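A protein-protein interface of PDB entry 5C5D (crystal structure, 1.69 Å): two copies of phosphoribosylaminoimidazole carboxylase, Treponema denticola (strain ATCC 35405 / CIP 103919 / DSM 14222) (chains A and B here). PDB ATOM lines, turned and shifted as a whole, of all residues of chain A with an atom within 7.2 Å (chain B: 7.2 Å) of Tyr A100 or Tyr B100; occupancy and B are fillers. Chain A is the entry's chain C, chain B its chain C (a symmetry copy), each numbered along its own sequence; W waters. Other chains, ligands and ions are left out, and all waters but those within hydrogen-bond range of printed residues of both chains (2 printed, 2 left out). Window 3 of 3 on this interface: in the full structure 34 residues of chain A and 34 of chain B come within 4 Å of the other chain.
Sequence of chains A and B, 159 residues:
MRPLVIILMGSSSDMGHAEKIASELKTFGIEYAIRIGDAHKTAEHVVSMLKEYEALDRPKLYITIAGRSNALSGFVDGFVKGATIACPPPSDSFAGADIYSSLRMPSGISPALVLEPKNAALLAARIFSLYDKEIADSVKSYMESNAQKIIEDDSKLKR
Printed residues of chain B that touch a printed residue of chain A: Tyr B100, Leu B103, Leu B113 and Leu B115. Hydrophobic or aromatic side chains of chain B within 4 Å of the printed part of chain A: Tyr B100, Leu B103, Leu B113 and Leu B115. Printed residues of chain A that touch a printed residue of chain B: Tyr A100, Leu A103, Leu A113 and Leu A115. Hydrophobic or aromatic side chains of chain A that line the printed part of chain B: Tyr A100, Leu A103, Leu A113 and Leu A115. Among the printed residues, no Asp or Glu carboxylate lies within 4 Å of a Lys or Arg side-chain nitrogen of the other chain.
Of chain B, only Tyr B100 comes within 4 Å of Tyr A100. Of the printed residues of chain B, Leu A103 touches Leu B113 and Leu B115. Met A105 touches none of the printed residues of chain B. Printed residues of chain B within 4 Å of Leu A113: Leu B103 and Leu B113. Of the printed residues of chain B, Leu A115 touches Leu B103. Gly B96 touches none of the printed residues of chain A. Of the printed residues of chain A, Leu B103 touches Leu A113 (3.9 Å) and Leu A115 (3.6 Å). Of the printed residues of chain A, Leu B115 touches Leu A103. The nearest residue of chain A that does not touch Tyr B100 is Ile A99 (4.5 Å). The nearest printed residue of chain B that does not touch Leu A103 is Ile B99 (4.2 Å).
Leu A103 touches Leu B113 (CD2 to CD2, 3.9 Å). Leu A103 touches Leu B115 (O to CD1, 3.6 Å). CD2 of Leu A113 touches CD2 of Leu B103 (3.9 Å). CD1 of Leu A115 touches O of Leu B103, at 3.6 Å.
Water W2 bridges the side-chain hydroxyl (OH) of Tyr A100 (2.6 Å) and the backbone carbonyl oxygen (O) of Ala B95 (3.1 Å). Water W1 bridges OH of Tyr B100 (2.6 Å) and O of Ala A95 (3.1 Å).
Tyr B100 touches its own counterpart, Tyr A100. Leu A103 touches Leu B113, and with the chains exchanged Leu A113 touches Leu B103. Leu A103 touches Leu B115, and with the chains exchanged Leu A115 touches Leu B103. Leu A113 touches its own counterpart, Leu B113. Of the 6 pairs that touch across the chains among the printed residues, 6 have their exchanged pair printed and touching as well.
OH of Tyr B100 lies within hydrogen-bond range of OH of Tyr A100. The backbone carbonyl oxygen (O) of Leu A113 is in hydrogen-bond range of the backbone NH (N) of Leu B113 (3.0 Å).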
ATOM      1  N   ASN A  70      -5.981  22.615 -12.887  1.00  0.00           N
ATOM      2  CA  ASN A  70      -4.792  22.647 -12.014  1.00  0.00           C
ATOM      3  C   ASN A  70      -3.955  21.407 -12.205  1.00  0.00           C
ATOM      4  O   ASN A  70      -4.247  20.332 -11.641  1.00  0.00           O
ATOM      5  CB  ASN A  70      -5.223  22.781 -10.569  1.00  0.00           C
ATOM      6  CG  ASN A  70      -4.062  22.725  -9.591  1.00  0.00           C
ATOM      7  OD1 ASN A  70      -2.892  22.759  -9.967  1.00  0.00           O
ATOM      8  ND2 ASN A  70      -4.391  22.605  -8.326  1.00  0.00           N
ATOM      9  N   PHE A  94     -18.007  27.691 -15.397  1.00  0.00           N
ATOM     10  CA  PHE A  94     -18.687  26.400 -15.353  1.00  0.00           C
ATOM     11  C   PHE A  94     -19.109  26.062 -13.920  1.00  0.00           C
ATOM     12  O   PHE A  94     -18.942  24.916 -13.456  1.00  0.00           O
ATOM     13  CB  PHE A  94     -17.771  25.311 -15.911  1.00  0.00           C
ATOM     14  CG  PHE A  94     -17.463  25.496 -17.375  1.00  0.00           C
ATOM     15  CD1 PHE A  94     -18.387  25.187 -18.319  1.00  0.00           C
ATOM     16  CD2 PHE A  94     -16.220  25.929 -17.774  1.00  0.00           C
ATOM     17  CE1 PHE A  94     -18.114  25.313 -19.657  1.00  0.00           C
ATOM     18  CE2 PHE A  94     -15.937  26.103 -19.115  1.00  0.00           C
ATOM     19  CZ  PHE A  94     -16.882  25.791 -20.059  1.00  0.00           C
ATOM     20  N   ALA A  95     -19.674  27.090 -13.278  1.00  0.00           N
ATOM     21  CA  ALA A  95     -20.147  26.999 -11.889  1.00  0.00           C
ATOM     22  C   ALA A  95     -19.127  26.374 -10.939  1.00  0.00           C
ATOM     23  O   ALA A  95     -19.447  25.546 -10.078  1.00  0.00           O
ATOM     24  CB  ALA A  95     -21.405  26.224 -11.842  1.00  0.00           C
ATOM     25  N   GLY A  96     -17.866  26.744 -11.117  1.00  0.00           N
ATOM     26  CA  GLY A  96     -16.822  26.292 -10.223  1.00  0.00           C
ATOM     27  C   GLY A  96     -16.183  24.959 -10.506  1.00  0.00           C
ATOM     28  O   GLY A  96     -15.383  24.474  -9.693  1.00  0.00           O
ATOM     29  N   ALA A  97     -16.477  24.395 -11.671  1.00  0.00           N
ATOM     30  CA  ALA A  97     -16.038  23.039 -11.980  1.00  0.00           C
ATOM     31  C   ALA A  97     -14.538  22.879 -12.126  1.00  0.00           C
ATOM     32  O   ALA A  97     -14.059  21.747 -12.128  1.00  0.00           O
ATOM     33  CB  ALA A  97     -16.734  22.549 -13.246  1.00  0.00           C
ATOM     34  N   ASP A  98     -13.770  23.974 -12.160  1.00  0.00           N
ATOM     35  CA  ASP A  98     -12.292  23.839 -12.110  1.00  0.00           C
ATOM     36  C   ASP A  98     -11.838  23.099 -10.828  1.00  0.00           C
ATOM     37  O   ASP A  98     -10.739  22.558 -10.767  1.00  0.00           O
ATOM     38  CB  ASP A  98     -11.586  25.211 -12.161  1.00  0.00           C
ATOM     39  CG  ASP A  98     -11.633  25.885 -13.517  1.00  0.00           C
ATOM     40  OD1 ASP A  98     -11.576  25.168 -14.536  1.00  0.00           O
ATOM     41  OD2 ASP A  98     -11.706  27.142 -13.575  1.00  0.00           O
ATOM     42  N   ILE A  99     -12.685  23.122  -9.795  1.00  0.00           N
ATOM     43  CA  ILE A  99     -12.329  22.464  -8.544  1.00  0.00           C
ATOM     44  C   ILE A  99     -12.035  20.960  -8.754  1.00  0.00           C
ATOM     45  O   ILE A  99     -11.181  20.401  -8.057  1.00  0.00           O
ATOM     46  CB  ILE A  99     -13.421  22.663  -7.477  1.00  0.00           C
ATOM     47  CG1 ILE A  99     -12.860  22.346  -6.059  1.00  0.00           C
ATOM     48  CG2 ILE A  99     -14.671  21.843  -7.766  1.00  0.00           C
ATOM     49  CD1 ILE A  99     -11.606  23.003  -5.652  1.00  0.00           C
ATOM     50  N   TYR A 100     -12.685  20.311  -9.706  1.00  0.00           N
ATOM     51  CA  TYR A 100     -12.488  18.865  -9.856  1.00  0.00           C
ATOM     52  C   TYR A 100     -11.075  18.520 -10.297  1.00  0.00           C
ATOM     53  O   TYR A 100     -10.601  17.422  -9.977  1.00  0.00           O
ATOM     54  CB  TYR A 100     -13.500  18.270 -10.817  1.00  0.00           C
ATOM     55  CG  TYR A 100     -14.885  18.315 -10.222  1.00  0.00           C
ATOM     56  CD1 TYR A 100     -15.225  17.410  -9.200  1.00  0.00           C
ATOM     57  CD2 TYR A 100     -15.788  19.287 -10.585  1.00  0.00           C
ATOM     58  CE1 TYR A 100     -16.477  17.466  -8.602  1.00  0.00           C
ATOM     59  CE2 TYR A 100     -17.047  19.344  -9.988  1.00  0.00           C
ATOM     60  CZ  TYR A 100     -17.357  18.423  -8.982  1.00  0.00           C
ATOM     61  OH  TYR A 100     -18.608  18.492  -8.399  1.00  0.00           O
ATOM     62  N   SER A 101     -10.393  19.434 -11.005  1.00  0.00           N
ATOM     63  CA  SER A 101      -9.009  19.194 -11.396  1.00  0.00           C
ATOM     64  C   SER A 101      -8.061  19.134 -10.221  1.00  0.00           C
ATOM     65  O   SER A 101      -6.998  18.517 -10.302  1.00  0.00           O
ATOM     66  CB  SER A 101      -8.529  20.242 -12.408  1.00  0.00           C
ATOM     67  OG  SER A 101      -8.464  21.546 -11.836  1.00  0.00           O
ATOM     68  N   SER A 102      -8.416  19.796  -9.130  1.00  0.00           N
ATOM     69  CA  SER A 102      -7.616  19.738  -7.912  1.00  0.00           C
ATOM     70  C   SER A 102      -7.961  18.513  -7.070  1.00  0.00           C
ATOM     71  O   SER A 102      -7.081  17.954  -6.407  1.00  0.00           O
ATOM     72  CB  SER A 102      -7.824  21.006  -7.082  1.00  0.00           C
ATOM     73  OG  SER A 102      -7.176  22.107  -7.708  1.00  0.00           O
ATOM     74  N   LEU A 103      -9.234  18.117  -7.086  1.00  0.00           N
ATOM     75  CA  LEU A 103      -9.748  16.989  -6.278  1.00  0.00           C
ATOM     76  C   LEU A 103      -9.287  15.617  -6.770  1.00  0.00           C
ATOM     77  O   LEU A 103      -8.909  14.755  -5.967  1.00  0.00           O
ATOM     78  CB  LEU A 103     -11.285  16.966  -6.257  1.00  0.00           C
ATOM     79  CG  LEU A 103     -12.123  17.937  -5.418  1.00  0.00           C
ATOM     80  CD1 LEU A 103     -13.541  17.927  -5.921  1.00  0.00           C
ATOM     81  CD2 LEU A 103     -12.097  17.476  -3.973  1.00  0.00           C
ATOM     82  N   ARG A 104      -9.347  15.408  -8.081  1.00  0.00           N
ATOM     83  CA  ARG A 104      -9.284  14.063  -8.667  1.00  0.00           C
ATOM     84  C   ARG A 104      -7.862  13.632  -9.003  1.00  0.00           C
ATOM     85  O   ARG A 104      -7.471  13.495 -10.148  1.00  0.00           O
ATOM     86  CB  ARG A 104     -10.171  14.020  -9.904  1.00  0.00           C
ATOM     87  CG  ARG A 104     -11.634  14.173  -9.522  1.00  0.00           C
ATOM     88  CD  ARG A 104     -12.279  12.844  -9.186  1.00  0.00           C
ATOM     89  NE  ARG A 104     -12.448  12.019 -10.374  1.00  0.00           N
ATOM     90  CZ  ARG A 104     -12.614  10.700 -10.394  1.00  0.00           C
ATOM     91  NH1 ARG A 104     -12.542   9.979  -9.255  1.00  0.00           N
ATOM     92  NH2 ARG A 104     -12.791  10.067 -11.543  1.00  0.00           N
ATOM     93  N   MET A 105      -7.123  13.349  -7.938  1.00  0.00           N
ATOM     94  CA  MET A 105      -5.764  12.870  -8.064  1.00  0.00           C
ATOM     95  C   MET A 105      -5.728  11.339  -8.227  1.00  0.00           C
ATOM     96  O   MET A 105      -6.606  10.629  -7.755  1.00  0.00           O
ATOM     97  CB  MET A 105      -4.969  13.310  -6.813  1.00  0.00           C
ATOM     98  CG  MET A 105      -4.907  14.777  -6.649  1.00  0.00           C
ATOM     99  SD  MET A 105      -3.948  15.560  -8.010  1.00  0.00           S
ATOM    100  CE  MET A 105      -5.254  16.110  -9.218  1.00  0.00           C
ATOM    101  N   LEU A 113      -6.245  19.462  -0.205  1.00  0.00           N
ATOM    102  CA  LEU A 113      -7.004  20.544  -0.846  1.00  0.00           C
ATOM    103  C   LEU A 113      -7.698  21.365   0.228  1.00  0.00           C
ATOM    104  O   LEU A 113      -8.393  20.798   1.098  1.00  0.00           O
ATOM    105  CB  LEU A 113      -8.033  19.989  -1.808  1.00  0.00           C
ATOM    106  CG  LEU A 113      -8.974  20.943  -2.560  1.00  0.00           C
ATOM    107  CD1 LEU A 113      -8.154  21.952  -3.368  1.00  0.00           C
ATOM    108  CD2 LEU A 113      -9.844  20.102  -3.439  1.00  0.00           C
ATOM    109  N   LEU A 115      -9.884  25.257   0.218  1.00  0.00           N
ATOM    110  CA  LEU A 115     -10.373  26.309  -0.663  1.00  0.00           C
ATOM    111  C   LEU A 115      -9.941  27.693  -0.229  1.00  0.00           C
ATOM    112  O   LEU A 115      -9.563  28.494  -1.063  1.00  0.00           O
ATOM    113  CB  LEU A 115     -11.909  26.303  -0.734  1.00  0.00           C
ATOM    114  CG  LEU A 115     -12.573  25.161  -1.474  1.00  0.00           C
ATOM    115  CD1 LEU A 115     -14.094  25.396  -1.477  1.00  0.00           C
ATOM    116  CD2 LEU A 115     -12.080  25.125  -2.883  1.00  0.00           C
ATOM    117  N   ASN B  70     -21.230  16.084   5.416  1.00  0.00           N
ATOM    118  CA  ASN B  70     -20.134  15.861   6.379  1.00  0.00           C
ATOM    119  C   ASN B  70     -20.018  17.021   7.334  1.00  0.00           C
ATOM    120  O   ASN B  70     -19.422  18.071   7.015  1.00  0.00           O
ATOM    121  CB  ASN B  70     -18.833  15.654   5.632  1.00  0.00           C
ATOM    122  CG  ASN B  70     -17.632  15.513   6.551  1.00  0.00           C
ATOM    123  OD1 ASN B  70     -17.755  15.391   7.769  1.00  0.00           O
ATOM    124  ND2 ASN B  70     -16.459  15.562   5.964  1.00  0.00           N
ATOM    125  N   PHE B  94     -26.715  12.474  -6.141  1.00  0.00           N
ATOM    126  CA  PHE B  94     -26.685  13.820  -6.707  1.00  0.00           C
ATOM    127  C   PHE B  94     -25.346  14.080  -7.403  1.00  0.00           C
ATOM    128  O   PHE B  94     -24.744  15.162  -7.249  1.00  0.00           O
ATOM    129  CB  PHE B  94     -26.924  14.852  -5.606  1.00  0.00           C
ATOM    130  CG  PHE B  94     -28.302  14.756  -5.000  1.00  0.00           C
ATOM    131  CD1 PHE B  94     -29.383  15.233  -5.667  1.00  0.00           C
ATOM    132  CD2 PHE B  94     -28.472  14.233  -3.740  1.00  0.00           C
ATOM    133  CE1 PHE B  94     -30.639  15.189  -5.119  1.00  0.00           C
ATOM    134  CE2 PHE B  94     -29.734  14.141  -3.185  1.00  0.00           C
ATOM    135  CZ  PHE B  94     -30.819  14.624  -3.872  1.00  0.00           C
ATOM    136  N   ALA B  95     -24.945  13.066  -8.177  1.00  0.00           N
ATOM    137  CA  ALA B  95     -23.685  13.091  -8.933  1.00  0.00           C
ATOM    138  C   ALA B  95     -22.483  13.530  -8.099  1.00  0.00           C
ATOM    139  O   ALA B  95     -21.630  14.313  -8.531  1.00  0.00           O
ATOM    140  CB  ALA B  95     -23.826  13.983 -10.104  1.00  0.00           C
ATOM    141  N   GLY B  96     -22.428  13.051  -6.864  1.00  0.00           N
ATOM    142  CA  GLY B  96     -21.293  13.320  -6.008  1.00  0.00           C
ATOM    143  C   GLY B  96     -21.299  14.600  -5.216  1.00  0.00           C
ATOM    144  O   GLY B  96     -20.291  14.934  -4.577  1.00  0.00           O
ATOM    145  N   ALA B  97     -22.437  15.284  -5.201  1.00  0.00           N
ATOM    146  CA  ALA B  97     -22.507  16.608  -4.596  1.00  0.00           C
ATOM    147  C   ALA B  97     -22.317  16.628  -3.092  1.00  0.00           C
ATOM    148  O   ALA B  97     -22.104  17.701  -2.534  1.00  0.00           O
ATOM    149  CB  ALA B  97     -23.835  17.268  -4.956  1.00  0.00           C
ATOM    150  N   ASP B  98     -22.300  15.467  -2.427  1.00  0.00           N
ATOM    151  CA  ASP B  98     -21.927  15.447  -0.991  1.00  0.00           C
ATOM    152  C   ASP B  98     -20.510  16.030  -0.769  1.00  0.00           C
ATOM    153  O   ASP B  98     -20.164  16.450   0.330  1.00  0.00           O
ATOM    154  CB  ASP B  98     -21.966  14.019  -0.404  1.00  0.00           C
ATOM    155  CG  ASP B  98     -23.363  13.466  -0.208  1.00  0.00           C
ATOM    156  OD1 ASP B  98     -24.269  14.254   0.129  1.00  0.00           O
ATOM    157  OD2 ASP B  98     -23.562  12.231  -0.369  1.00  0.00           O
ATOM    158  N   ILE B  99     -19.686  16.010  -1.821  1.00  0.00           N
ATOM    159  CA  ILE B  99     -18.328  16.524  -1.695  1.00  0.00           C
ATOM    160  C   ILE B  99     -18.317  18.002  -1.241  1.00  0.00           C
ATOM    161  O   ILE B  99     -17.404  18.414  -0.518  1.00  0.00           O
ATOM    162  CB  ILE B  99     -17.540  16.350  -3.007  1.00  0.00           C
ATOM    163  CG1 ILE B  99     -16.012  16.493  -2.746  1.00  0.00           C
ATOM    164  CG2 ILE B  99     -18.002  17.313  -4.092  1.00  0.00           C
ATOM    165  CD1 ILE B  99     -15.418  15.681  -1.669  1.00  0.00           C
ATOM    166  N   TYR B 100     -19.315  18.789  -1.611  1.00  0.00           N
ATOM    167  CA  TYR B 100     -19.273  20.215  -1.270  1.00  0.00           C
ATOM    168  C   TYR B 100     -19.368  20.450   0.229  1.00  0.00           C
ATOM    169  O   TYR B 100     -18.847  21.464   0.709  1.00  0.00           O
ATOM    170  CB  TYR B 100     -20.360  20.986  -1.995  1.00  0.00           C
ATOM    171  CG  TYR B 100     -20.077  21.033  -3.476  1.00  0.00           C
ATOM    172  CD1 TYR B 100     -19.063  21.882  -3.956  1.00  0.00           C
ATOM    173  CD2 TYR B 100     -20.718  20.191  -4.353  1.00  0.00           C
ATOM    174  CE1 TYR B 100     -18.750  21.904  -5.309  1.00  0.00           C
ATOM    175  CE2 TYR B 100     -20.409  20.213  -5.713  1.00  0.00           C
ATOM    176  CZ  TYR B 100     -19.403  21.076  -6.160  1.00  0.00           C
ATOM    177  OH  TYR B 100     -19.106  21.086  -7.509  1.00  0.00           O
ATOM    178  N   SER B 101     -20.006  19.532   0.972  1.00  0.00           N
ATOM    179  CA  SER B 101     -20.071  19.662   2.424  1.00  0.00           C
ATOM    180  C   SER B 101     -18.723  19.529   3.093  1.00  0.00           C
ATOM    181  O   SER B 101     -18.515  20.040   4.195  1.00  0.00           O
ATOM    182  CB  SER B 101     -21.060  18.656   3.026  1.00  0.00           C
ATOM    183  OG  SER B 101     -20.622  17.311   2.859  1.00  0.00           O
ATOM    184  N   SER B 102     -17.804  18.820   2.455  1.00  0.00           N
ATOM    185  CA  SER B 102     -16.445  18.698   2.971  1.00  0.00           C
ATOM    186  C   SER B 102     -15.575  19.879   2.550  1.00  0.00           C
ATOM    187  O   SER B 102     -14.688  20.290   3.307  1.00  0.00           O
ATOM    188  CB  SER B 102     -15.810  17.394   2.484  1.00  0.00           C
ATOM    189  OG  SER B 102     -16.394  16.288   3.161  1.00  0.00           O
ATOM    190  N   LEU B 103     -15.818  20.401   1.349  1.00  0.00           N
ATOM    191  CA  LEU B 103     -15.027  21.506   0.764  1.00  0.00           C
ATOM    192  C   LEU B 103     -15.269  22.860   1.432  1.00  0.00           C
ATOM    193  O   LEU B 103     -14.321  23.611   1.693  1.00  0.00           O
ATOM    194  CB  LEU B 103     -15.327  21.683  -0.734  1.00  0.00           C
ATOM    195  CG  LEU B 103     -14.786  20.737  -1.811  1.00  0.00           C
ATOM    196  CD1 LEU B 103     -15.572  20.931  -3.079  1.00  0.00           C
ATOM    197  CD2 LEU B 103     -13.329  21.074  -2.065  1.00  0.00           C
ATOM    198  N   ARG B 104     -16.535  23.180   1.677  1.00  0.00           N
ATOM    199  CA  ARG B 104     -16.955  24.555   1.976  1.00  0.00           C
ATOM    200  C   ARG B 104     -16.939  24.866   3.467  1.00  0.00           C
ATOM    201  O   ARG B 104     -17.956  25.055   4.110  1.00  0.00           O
ATOM    202  CB  ARG B 104     -18.340  24.789   1.388  1.00  0.00           C
ATOM    203  CG  ARG B 104     -18.293  24.754  -0.130  1.00  0.00           C
ATOM    204  CD  ARG B 104     -17.967  26.109  -0.723  1.00  0.00           C
ATOM    205  NE  ARG B 104     -19.074  27.041  -0.560  1.00  0.00           N
ATOM    206  CZ  ARG B 104     -18.994  28.368  -0.610  1.00  0.00           C
ATOM    207  NH1 ARG B 104     -17.799  28.982  -0.730  1.00  0.00           N
ATOM    208  NH2 ARG B 104     -20.085  29.106  -0.479  1.00  0.00           N
ATOM    209  N   MET B 105     -15.720  24.985   3.976  1.00  0.00           N
ATOM    210  CA  MET B 105     -15.507  25.333   5.364  1.00  0.00           C
ATOM    211  C   MET B 105     -15.504  26.860   5.559  1.00  0.00           C
ATOM    212  O   MET B 105     -15.157  27.614   4.660  1.00  0.00           O
ATOM    213  CB  MET B 105     -14.169  24.714   5.827  1.00  0.00           C
ATOM    214  CG  MET B 105     -14.144  23.240   5.732  1.00  0.00           C
ATOM    215  SD  MET B 105     -15.345  22.477   6.898  1.00  0.00           S
ATOM    216  CE  MET B 105     -16.850  22.162   5.848  1.00  0.00           C
ATOM    217  N   LEU B 113      -8.635  18.205   2.639  1.00  0.00           N
ATOM    218  CA  LEU B 113      -9.528  17.262   1.954  1.00  0.00           C
ATOM    219  C   LEU B 113      -8.712  16.431   0.976  1.00  0.00           C
ATOM    220  O   LEU B 113      -7.955  16.993   0.157  1.00  0.00           O
ATOM    221  CB  LEU B 113     -10.623  17.995   1.208  1.00  0.00           C
ATOM    222  CG  LEU B 113     -11.649  17.205   0.381  1.00  0.00           C
ATOM    223  CD1 LEU B 113     -12.364  16.188   1.273  1.00  0.00           C
ATOM    224  CD2 LEU B 113     -12.601  18.198  -0.205  1.00  0.00           C
ATOM    225  N   LEU B 115      -9.576  12.794  -1.463  1.00  0.00           N
ATOM    226  CA  LEU B 115     -10.642  11.872  -1.832  1.00  0.00           C
ATOM    227  C   LEU B 115     -10.270  10.421  -1.620  1.00  0.00           C
ATOM    228  O   LEU B 115     -11.082   9.656  -1.135  1.00  0.00           O
ATOM    229  CB  LEU B 115     -11.034  12.039  -3.309  1.00  0.00           C
ATOM    230  CG  LEU B 115     -11.777  13.299  -3.700  1.00  0.00           C
ATOM    231  CD1 LEU B 115     -12.124  13.221  -5.198  1.00  0.00           C
ATOM    232  CD2 LEU B 115     -13.040  13.399  -2.909  1.00  0.00           C
HETATM  233  O   HOH W   1     -18.949  22.485  -9.720  1.00  0.00           O
HETATM  234  O   HOH W   2     -20.867  17.269  -7.876  1.00  0.00           O
